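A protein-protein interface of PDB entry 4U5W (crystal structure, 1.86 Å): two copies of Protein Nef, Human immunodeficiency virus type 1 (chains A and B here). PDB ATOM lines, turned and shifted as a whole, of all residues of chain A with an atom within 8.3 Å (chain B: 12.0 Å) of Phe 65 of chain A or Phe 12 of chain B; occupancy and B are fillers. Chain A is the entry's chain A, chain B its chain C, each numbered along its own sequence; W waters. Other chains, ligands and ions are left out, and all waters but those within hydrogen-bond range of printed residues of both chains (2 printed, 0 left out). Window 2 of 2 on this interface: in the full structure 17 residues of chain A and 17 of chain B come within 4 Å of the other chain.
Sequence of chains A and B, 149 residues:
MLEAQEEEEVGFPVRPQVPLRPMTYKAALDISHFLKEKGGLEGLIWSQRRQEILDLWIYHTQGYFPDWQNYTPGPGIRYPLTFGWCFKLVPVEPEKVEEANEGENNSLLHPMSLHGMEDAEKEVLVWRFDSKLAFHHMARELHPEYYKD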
ATOM      1  N   GLN A  17      -0.056   8.860   6.133  1.00  0.00           N
ATOM      2  CA  GLN A  17       0.424  10.192   5.795  1.00  0.00           C
ATOM      3  C   GLN A  17       0.750  10.315   4.303  1.00  0.00           C
ATOM      4  O   GLN A  17       1.453   9.472   3.755  1.00  0.00           O
ATOM      5  CB  GLN A  17       1.676  10.513   6.619  1.00  0.00           C
ATOM      6  CG  GLN A  17       2.274  11.863   6.303  1.00  0.00           C
ATOM      7  CD  GLN A  17       1.344  12.980   6.684  1.00  0.00           C
ATOM      8  OE1 GLN A  17       0.879  13.048   7.822  1.00  0.00           O
ATOM      9  NE2 GLN A  17       1.047  13.857   5.734  1.00  0.00           N
ATOM     10  N   PRO A  19       2.331  12.594   0.908  1.00  0.00           N
ATOM     11  CA  PRO A  19       3.541  13.418   0.798  1.00  0.00           C
ATOM     12  C   PRO A  19       3.289  14.917   1.003  1.00  0.00           C
ATOM     13  O   PRO A  19       2.193  15.416   0.741  1.00  0.00           O
ATOM     14  CB  PRO A  19       4.020  13.146  -0.632  1.00  0.00           C
ATOM     15  CG  PRO A  19       3.421  11.833  -1.006  1.00  0.00           C
ATOM     16  CD  PRO A  19       2.069  11.841  -0.329  1.00  0.00           C
ATOM     17  N   LEU A  20       4.317  15.618   1.472  1.00  0.00           N
ATOM     18  CA  LEU A  20       4.237  17.054   1.707  1.00  0.00           C
ATOM     19  C   LEU A  20       4.030  17.837   0.423  1.00  0.00           C
ATOM     20  O   LEU A  20       4.589  17.496  -0.625  1.00  0.00           O
ATOM     21  CB  LEU A  20       5.513  17.554   2.389  1.00  0.00           C
ATOM     22  CG  LEU A  20       5.766  17.158   3.843  1.00  0.00           C
ATOM     23  CD1 LEU A  20       7.183  17.556   4.242  1.00  0.00           C
ATOM     24  CD2 LEU A  20       4.749  17.827   4.748  1.00  0.00           C
ATOM     25  N   ARG A  21       3.243  18.900   0.512  1.00  0.00           N
ATOM     26  CA  ARG A  21       3.129  19.864  -0.578  1.00  0.00           C
ATOM     27  C   ARG A  21       2.724  21.213   0.014  1.00  0.00           C
ATOM     28  O   ARG A  21       2.095  21.249   1.077  1.00  0.00           O
ATOM     29  CB  ARG A  21       2.125  19.384  -1.625  1.00  0.00           C
ATOM     30  CG  ARG A  21       0.774  18.925  -1.059  1.00  0.00           C
ATOM     31  CD  ARG A  21      -0.221  18.613  -2.179  1.00  0.00           C
ATOM     32  NE  ARG A  21      -1.444  17.993  -1.656  1.00  0.00           N
ATOM     33  CZ  ARG A  21      -2.473  17.618  -2.403  1.00  0.00           C
ATOM     34  NH1 ARG A  21      -2.453  17.819  -3.715  1.00  0.00           N
ATOM     35  NH2 ARG A  21      -3.532  17.055  -1.833  1.00  0.00           N
ATOM     36  N   PRO A  22       3.082  22.327  -0.653  1.00  0.00           N
ATOM     37  CA  PRO A  22       2.821  23.634  -0.038  1.00  0.00           C
ATOM     38  C   PRO A  22       1.365  24.063  -0.147  1.00  0.00           C
ATOM     39  O   PRO A  22       0.687  23.710  -1.113  1.00  0.00           O
ATOM     40  CB  PRO A  22       3.713  24.587  -0.843  1.00  0.00           C
ATOM     41  CG  PRO A  22       3.778  23.966  -2.202  1.00  0.00           C
ATOM     42  CD  PRO A  22       3.756  22.457  -1.963  1.00  0.00           C
ATOM     43  N   MET A  23       0.893  24.829   0.829  1.00  0.00           N
ATOM     44  CA  MET A  23      -0.460  25.377   0.763  1.00  0.00           C
ATOM     45  C   MET A  23      -0.487  26.423  -0.349  1.00  0.00           C
ATOM     46  O   MET A  23       0.488  27.148  -0.540  1.00  0.00           O
ATOM     47  CB  MET A  23      -0.873  25.977   2.115  1.00  0.00           C
ATOM     48  CG  MET A  23      -2.208  26.736   2.106  1.00  0.00           C
ATOM     49  SD  MET A  23      -3.576  25.728   1.509  1.00  0.00           S
ATOM     50  CE  MET A  23      -3.692  24.462   2.778  1.00  0.00           C
ATOM     51  N   ASP A  55      -6.497  20.838  11.525  1.00  0.00           N
ATOM     52  CA  ASP A  55      -5.217  21.017  10.834  1.00  0.00           C
ATOM     53  C   ASP A  55      -4.432  19.712  10.715  1.00  0.00           C
ATOM     54  O   ASP A  55      -3.769  19.472   9.700  1.00  0.00           O
ATOM     55  CB  ASP A  55      -4.369  22.070  11.545  1.00  0.00           C
ATOM     56  CG  ASP A  55      -4.820  23.489  11.227  1.00  0.00           C
ATOM     57  OD1 ASP A  55      -5.583  23.668  10.254  1.00  0.00           O
ATOM     58  OD2 ASP A  55      -4.411  24.423  11.945  1.00  0.00           O
ATOM     59  N   LEU A  56      -4.507  18.865  11.742  1.00  0.00           N
ATOM     60  CA  LEU A  56      -3.801  17.590  11.700  1.00  0.00           C
ATOM     61  C   LEU A  56      -4.439  16.686  10.654  1.00  0.00           C
ATOM     62  O   LEU A  56      -3.748  15.987   9.912  1.00  0.00           O
ATOM     63  CB  LEU A  56      -3.807  16.916  13.084  1.00  0.00           C
ATOM     64  CG  LEU A  56      -3.011  15.621  13.314  1.00  0.00           C
ATOM     65  CD1 LEU A  56      -3.767  14.376  12.847  1.00  0.00           C
ATOM     66  CD2 LEU A  56      -1.637  15.710  12.654  1.00  0.00           C
ATOM     67  N   ILE A  58      -6.118  17.558   7.966  1.00  0.00           N
ATOM     68  CA  ILE A  58      -5.736  18.088   6.658  1.00  0.00           C
ATOM     69  C   ILE A  58      -4.299  17.718   6.300  1.00  0.00           C
ATOM     70  O   ILE A  58      -4.015  17.306   5.178  1.00  0.00           O
ATOM     71  CB  ILE A  58      -5.923  19.610   6.633  1.00  0.00           C
ATOM     72  CG1 ILE A  58      -7.423  19.915   6.657  1.00  0.00           C
ATOM     73  CG2 ILE A  58      -5.258  20.230   5.394  1.00  0.00           C
ATOM     74  CD1 ILE A  58      -7.768  21.385   6.883  1.00  0.00           C
ATOM     75  N   TYR A  59      -3.396  17.854   7.263  1.00  0.00           N
ATOM     76  CA  TYR A  59      -1.998  17.492   7.047  1.00  0.00           C
ATOM     77  C   TYR A  59      -1.850  16.008   6.718  1.00  0.00           C
ATOM     78  O   TYR A  59      -1.220  15.634   5.724  1.00  0.00           O
ATOM     79  CB  TYR A  59      -1.161  17.843   8.282  1.00  0.00           C
ATOM     80  CG  TYR A  59       0.231  17.262   8.227  1.00  0.00           C
ATOM     81  CD1 TYR A  59       1.171  17.762   7.332  1.00  0.00           C
ATOM     82  CD2 TYR A  59       0.604  16.203   9.045  1.00  0.00           C
ATOM     83  CE1 TYR A  59       2.447  17.235   7.265  1.00  0.00           C
ATOM     84  CE2 TYR A  59       1.888  15.662   8.981  1.00  0.00           C
ATOM     85  CZ  TYR A  59       2.801  16.184   8.092  1.00  0.00           C
ATOM     86  OH  TYR A  59       4.076  15.665   8.018  1.00  0.00           O
ATOM     87  N   HIS A  60      -2.444  15.159   7.551  1.00  0.00           N
ATOM     88  CA  HIS A  60      -2.336  13.719   7.371  1.00  0.00           C
ATOM     89  C   HIS A  60      -2.878  13.286   6.014  1.00  0.00           C
ATOM     90  O   HIS A  60      -2.224  12.543   5.283  1.00  0.00           O
ATOM     91  CB  HIS A  60      -3.091  12.990   8.493  1.00  0.00           C
ATOM     92  CG  HIS A  60      -3.027  11.497   8.410  1.00  0.00           C
ATOM     93  ND1 HIS A  60      -2.585  10.714   9.460  1.00  0.00           N
ATOM     94  CD2 HIS A  60      -3.401  10.627   7.439  1.00  0.00           C
ATOM     95  CE1 HIS A  60      -2.658   9.441   9.128  1.00  0.00           C
ATOM     96  NE2 HIS A  60      -3.154   9.358   7.903  1.00  0.00           N
ATOM     97  N   GLN A  62      -3.994  15.203   3.333  1.00  0.00           N
ATOM     98  CA  GLN A  62      -3.824  16.019   2.133  1.00  0.00           C
ATOM     99  C   GLN A  62      -2.409  16.601   1.973  1.00  0.00           C
ATOM    100  O   GLN A  62      -2.044  17.038   0.886  1.00  0.00           O
ATOM    101  CB  GLN A  62      -4.867  17.148   2.105  1.00  0.00           C
ATOM    102  CG  GLN A  62      -6.325  16.641   2.041  1.00  0.00           C
ATOM    103  CD  GLN A  62      -6.610  15.811   0.793  1.00  0.00           C
ATOM    104  OE1 GLN A  62      -6.015  16.028  -0.261  1.00  0.00           O
ATOM    105  NE2 GLN A  62      -7.512  14.851   0.914  1.00  0.00           N
ATOM    106  N   GLY A  63      -1.621  16.610   3.042  1.00  0.00           N
ATOM    107  CA  GLY A  63      -0.197  16.906   2.928  1.00  0.00           C
ATOM    108  C   GLY A  63       0.264  18.328   3.181  1.00  0.00           C
ATOM    109  O   GLY A  63       1.440  18.646   2.987  1.00  0.00           O
ATOM    110  N   TYR A  64      -0.649  19.189   3.618  1.00  0.00           N
ATOM    111  CA  TYR A  64      -0.313  20.583   3.882  1.00  0.00           C
ATOM    112  C   TYR A  64       0.153  20.782   5.318  1.00  0.00           C
ATOM    113  O   TYR A  64      -0.610  20.531   6.256  1.00  0.00           O
ATOM    114  CB  TYR A  64      -1.524  21.480   3.577  1.00  0.00           C
ATOM    115  CG  TYR A  64      -2.027  21.291   2.162  1.00  0.00           C
ATOM    116  CD1 TYR A  64      -1.274  21.730   1.076  1.00  0.00           C
ATOM    117  CD2 TYR A  64      -3.236  20.653   1.908  1.00  0.00           C
ATOM    118  CE1 TYR A  64      -1.716  21.544  -0.227  1.00  0.00           C
ATOM    119  CE2 TYR A  64      -3.691  20.471   0.603  1.00  0.00           C
ATOM    120  CZ  TYR A  64      -2.924  20.919  -0.455  1.00  0.00           C
ATOM    121  OH  TYR A  64      -3.360  20.739  -1.752  1.00  0.00           O
ATOM    122  N   PHE A  65       1.398  21.233   5.486  1.00  0.00           N
ATOM    123  CA  PHE A  65       1.934  21.533   6.818  1.00  0.00           C
ATOM    124  C   PHE A  65       0.985  22.475   7.547  1.00  0.00           C
ATOM    125  O   PHE A  65       0.545  23.461   6.966  1.00  0.00           O
ATOM    126  CB  PHE A  65       3.315  22.175   6.738  1.00  0.00           C
ATOM    127  CG  PHE A  65       4.033  22.218   8.055  1.00  0.00           C
ATOM    128  CD1 PHE A  65       3.854  23.281   8.926  1.00  0.00           C
ATOM    129  CD2 PHE A  65       4.889  21.179   8.427  1.00  0.00           C
ATOM    130  CE1 PHE A  65       4.509  23.310  10.149  1.00  0.00           C
ATOM    131  CE2 PHE A  65       5.543  21.206   9.640  1.00  0.00           C
ATOM    132  CZ  PHE A  65       5.353  22.275  10.503  1.00  0.00           C
ATOM    133  N   PRO A  66       0.674  22.169   8.815  1.00  0.00           N
ATOM    134  CA  PRO A  66      -0.376  22.864   9.575  1.00  0.00           C
ATOM    135  C   PRO A  66       0.036  24.195  10.201  1.00  0.00           C
ATOM    136  O   PRO A  66      -0.050  24.335  11.419  1.00  0.00           O
ATOM    137  CB  PRO A  66      -0.726  21.856  10.672  1.00  0.00           C
ATOM    138  CG  PRO A  66       0.547  21.116  10.906  1.00  0.00           C
ATOM    139  CD  PRO A  66       1.180  20.988   9.534  1.00  0.00           C
ATOM    140  N   ASP A  67       0.447  25.161   9.383  1.00  0.00           N
ATOM    141  CA  ASP A  67       0.679  26.514   9.873  1.00  0.00           C
ATOM    142  C   ASP A  67       0.037  27.565   8.956  1.00  0.00           C
ATOM    143  O   ASP A  67       0.470  28.714   8.921  1.00  0.00           O
ATOM    144  CB  ASP A  67       2.180  26.774  10.012  1.00  0.00           C
ATOM    145  CG  ASP A  67       2.897  26.788   8.674  1.00  0.00           C
ATOM    146  OD1 ASP A  67       2.284  26.399   7.656  1.00  0.00           O
ATOM    147  OD2 ASP A  67       4.082  27.178   8.641  1.00  0.00           O
ATOM    148  N   TRP A  68      -0.988  27.161   8.213  1.00  0.00           N
ATOM    149  CA  TRP A  68      -1.618  28.032   7.225  1.00  0.00           C
ATOM    150  C   TRP A  68      -2.917  28.643   7.730  1.00  0.00           C
ATOM    151  O   TRP A  68      -3.365  29.663   7.221  1.00  0.00           O
ATOM    152  CB  TRP A  68      -1.907  27.259   5.941  1.00  0.00           C
ATOM    153  CG  TRP A  68      -2.772  26.070   6.193  1.00  0.00           C
ATOM    154  CD1 TRP A  68      -2.353  24.800   6.494  1.00  0.00           C
ATOM    155  CD2 TRP A  68      -4.203  26.036   6.206  1.00  0.00           C
ATOM    156  NE1 TRP A  68      -3.436  23.979   6.675  1.00  0.00           N
ATOM    157  CE2 TRP A  68      -4.582  24.711   6.509  1.00  0.00           C
ATOM    158  CE3 TRP A  68      -5.199  26.994   5.982  1.00  0.00           C
ATOM    159  CZ2 TRP A  68      -5.917  24.323   6.597  1.00  0.00           C
ATOM    160  CZ3 TRP A  68      -6.523  26.606   6.071  1.00  0.00           C
ATOM    161  CH2 TRP A  68      -6.872  25.282   6.376  1.00  0.00           C
ATOM    162  N   GLN A  69      -3.535  28.005   8.717  1.00  0.00           N
ATOM    163  CA  GLN A  69      -4.843  28.453   9.184  1.00  0.00           C
ATOM    164  C   GLN A  69      -4.743  29.461  10.318  1.00  0.00           C
ATOM    165  O   GLN A  69      -5.066  29.155  11.467  1.00  0.00           O
ATOM    166  CB  GLN A  69      -5.698  27.261   9.635  1.00  0.00           C
ATOM    167  CG  GLN A  69      -7.188  27.583   9.572  1.00  0.00           C
ATOM    168  CD  GLN A  69      -8.060  26.597  10.320  1.00  0.00           C
ATOM    169  OE1 GLN A  69      -9.143  26.950  10.788  1.00  0.00           O
ATOM    170  NE2 GLN A  69      -7.604  25.356  10.428  1.00  0.00           N
ATOM    171  N   GLY B  11       5.789  21.431  17.379  1.00  0.00           N
ATOM    172  CA  GLY B  11       6.293  22.320  16.346  1.00  0.00           C
ATOM    173  C   GLY B  11       6.569  21.617  15.030  1.00  0.00           C
ATOM    174  O   GLY B  11       5.645  21.243  14.307  1.00  0.00           O
ATOM    175  N   PHE B  12       7.845  21.427  14.720  1.00  0.00           N
ATOM    176  CA  PHE B  12       8.213  20.718  13.503  1.00  0.00           C
ATOM    177  C   PHE B  12       9.331  19.699  13.741  1.00  0.00           C
ATOM    178  O   PHE B  12      10.165  19.886  14.627  1.00  0.00           O
ATOM    179  CB  PHE B  12       8.630  21.708  12.420  1.00  0.00           C
ATOM    180  CG  PHE B  12       9.949  22.385  12.683  1.00  0.00           C
ATOM    181  CD1 PHE B  12      11.124  21.864  12.173  1.00  0.00           C
ATOM    182  CD2 PHE B  12      10.011  23.546  13.429  1.00  0.00           C
ATOM    183  CE1 PHE B  12      12.333  22.480  12.400  1.00  0.00           C
ATOM    184  CE2 PHE B  12      11.227  24.180  13.657  1.00  0.00           C
ATOM    185  CZ  PHE B  12      12.390  23.635  13.149  1.00  0.00           C
ATOM    186  N   PRO B  13       9.345  18.602  12.959  1.00  0.00           N
ATOM    187  CA  PRO B  13       8.292  18.209  12.010  1.00  0.00           C
ATOM    188  C   PRO B  13       7.010  17.836  12.747  1.00  0.00           C
ATOM    189  O   PRO B  13       7.046  17.701  13.969  1.00  0.00           O
ATOM    190  CB  PRO B  13       8.883  16.983  11.301  1.00  0.00           C
ATOM    191  CG  PRO B  13      10.358  17.029  11.596  1.00  0.00           C
ATOM    192  CD  PRO B  13      10.470  17.650  12.945  1.00  0.00           C
ATOM    193  N   VAL B  14       5.896  17.701  12.032  1.00  0.00           N
ATOM    194  CA  VAL B  14       4.651  17.288  12.664  1.00  0.00           C
ATOM    195  C   VAL B  14       4.829  15.894  13.259  1.00  0.00           C
ATOM    196  O   VAL B  14       5.444  15.022  12.646  1.00  0.00           O
ATOM    197  CB  VAL B  14       3.476  17.294  11.666  1.00  0.00           C
ATOM    198  CG1 VAL B  14       2.188  16.850  12.347  1.00  0.00           C
ATOM    199  CG2 VAL B  14       3.310  18.684  11.061  1.00  0.00           C
ATOM    200  N   ARG B  15       4.316  15.688  14.466  1.00  0.00           N
ATOM    201  CA  ARG B  15       4.455  14.388  15.108  1.00  0.00           C
ATOM    202  C   ARG B  15       3.762  13.324  14.251  1.00  0.00           C
ATOM    203  O   ARG B  15       2.642  13.524  13.780  1.00  0.00           O
ATOM    204  CB  ARG B  15       3.896  14.431  16.530  1.00  0.00           C
ATOM    205  CG  ARG B  15       2.398  14.600  16.608  1.00  0.00           C
ATOM    206  CD  ARG B  15       1.979  15.104  17.980  1.00  0.00           C
ATOM    207  NE  ARG B  15       2.336  16.509  18.164  1.00  0.00           N
ATOM    208  CZ  ARG B  15       2.177  17.173  19.303  1.00  0.00           C
ATOM    209  NH1 ARG B  15       1.673  16.554  20.363  1.00  0.00           N
ATOM    210  NH2 ARG B  15       2.527  18.449  19.383  1.00  0.00           N
ATOM    211  N   PRO B  16       4.458  12.206  13.991  1.00  0.00           N
ATOM    212  CA  PRO B  16       3.913  11.242  13.033  1.00  0.00           C
ATOM    213  C   PRO B  16       2.964  10.208  13.658  1.00  0.00           C
ATOM    214  O   PRO B  16       2.681  10.244  14.856  1.00  0.00           O
ATOM    215  CB  PRO B  16       5.170  10.561  12.488  1.00  0.00           C
ATOM    216  CG  PRO B  16       6.092  10.541  13.692  1.00  0.00           C
ATOM    217  CD  PRO B  16       5.835  11.864  14.404  1.00  0.00           C
ATOM    218  N   HIS B  60      -4.046   8.718  14.734  1.00  0.00           N
ATOM    219  CA  HIS B  60      -2.728   9.254  14.369  1.00  0.00           C
ATOM    220  C   HIS B  60      -1.881   9.545  15.611  1.00  0.00           C
ATOM    221  O   HIS B  60      -0.718   9.142  15.692  1.00  0.00           O
ATOM    222  CB  HIS B  60      -2.890  10.533  13.514  1.00  0.00           C
ATOM    223  CG  HIS B  60      -1.598  11.198  13.136  1.00  0.00           C
ATOM    224  ND1 HIS B  60      -1.280  11.503  11.826  1.00  0.00           N
ATOM    225  CD2 HIS B  60      -0.569  11.671  13.880  1.00  0.00           C
ATOM    226  CE1 HIS B  60      -0.109  12.105  11.779  1.00  0.00           C
ATOM    227  NE2 HIS B  60       0.350  12.222  13.018  1.00  0.00           N
HETATM  228  O   HOH W   1       4.672  13.654   9.567  1.00  0.00           O
HETATM  229  O   HOH W   2       6.212  17.461   9.006  1.00  0.00           O
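A ring nitrogen (ND1) of His 60 of chain B is in hydrogen-bond range of a ring nitrogen (ND1) of His 60 of chain A, 2.8 Å away.
The side-chain amide nitrogen of Gln 17 of chain A sits at hydrogen-bond distance from the backbone carbonyl oxygen of Tyr 59 of chain A (2.9 Å).
The backbone carbonyl oxygen of Arg 15 of chain B sits at hydrogen-bond distance from a ring nitrogen (NE2) of His 60 of chain B (2.7 Å).
Among the printed residues, merely in contact across the chains: Leu 56 of chain A with His 60 of chain B, Tyr 59 of chain A with Val 14 of chain B, Phe 65 of chain A with Gly 11 of chain B, Phe 65 of chain A with Phe 12 of chain B, Phe 65 of chain A with Val 14 of chain B and Pro 66 of chain A with Val 14 of chain B.
No residue of chain B comes within 4 Å of Leu 20 of chain A.
Of the printed residues of chain B, Leu 56 of chain A touches His 60.
Of the printed residues of chain B, His 60 of chain A touches His 60 (2.8 Å).
Trp 68 of chain A touches none of the printed residues of chain B.
Of chain A, only Phe 65 (3.95 Å) comes within 4 Å of Gly 11 of chain B.
Of the printed residues of chain A, Phe 12 of chain B touches Phe 65 (3.8 Å).
No residue of chain A comes within 4 Å of Pro 13 of chain B.
Of the printed residues of chain A, Val 14 of chain B touches Tyr 59, Phe 65 and Pro 66.
The nearest residue of chain B that does not touch Phe 65 of chain A is Pro 13 of chain B (4.7 Å).
The nearest printed residue of chain A that does not touch His 60 of chain B is Gln 17 of chain A (4.2 Å).
Of the 7 printed residues of chain B, 4 touch a printed residue of chain A.
Hydrophobic or aromatic side chains of chain B within 4 Å of the printed part of chain A: Phe 12, Val 14 and His 60.
Of the 19 printed residues of chain A, 5 touch a printed residue of chain B.
Hydrophobic or aromatic side chains of chain A that line the printed part of chain B: Leu 56, Tyr 59, His 60, Phe 65 and Pro 66.
Along chain A the printed residues that touch a printed residue of chain B span positions 56 to 66.
Among the printed residues, no Asp or Glu carboxylate lies within 4 Å of a Lys or Arg side-chain nitrogen of the other chain.
His 60 of chain A touches its own counterpart, His 60 of chain B.
Position printed for both chains: 60.
Of the 7 pairs that touch across the chains among the printed residues, 1 has its exchanged pair printed and touching as well.
Water W1 lies within hydrogen-bond range of OH of Tyr 59 of chain A and O of Val 14 of chain B.
Water W2 bridges the side-chain hydroxyl (OH) of Tyr 59 of chain A (3.0 Å) and the backbone NH (N) of Val 14 of chain B (3.1 Å).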
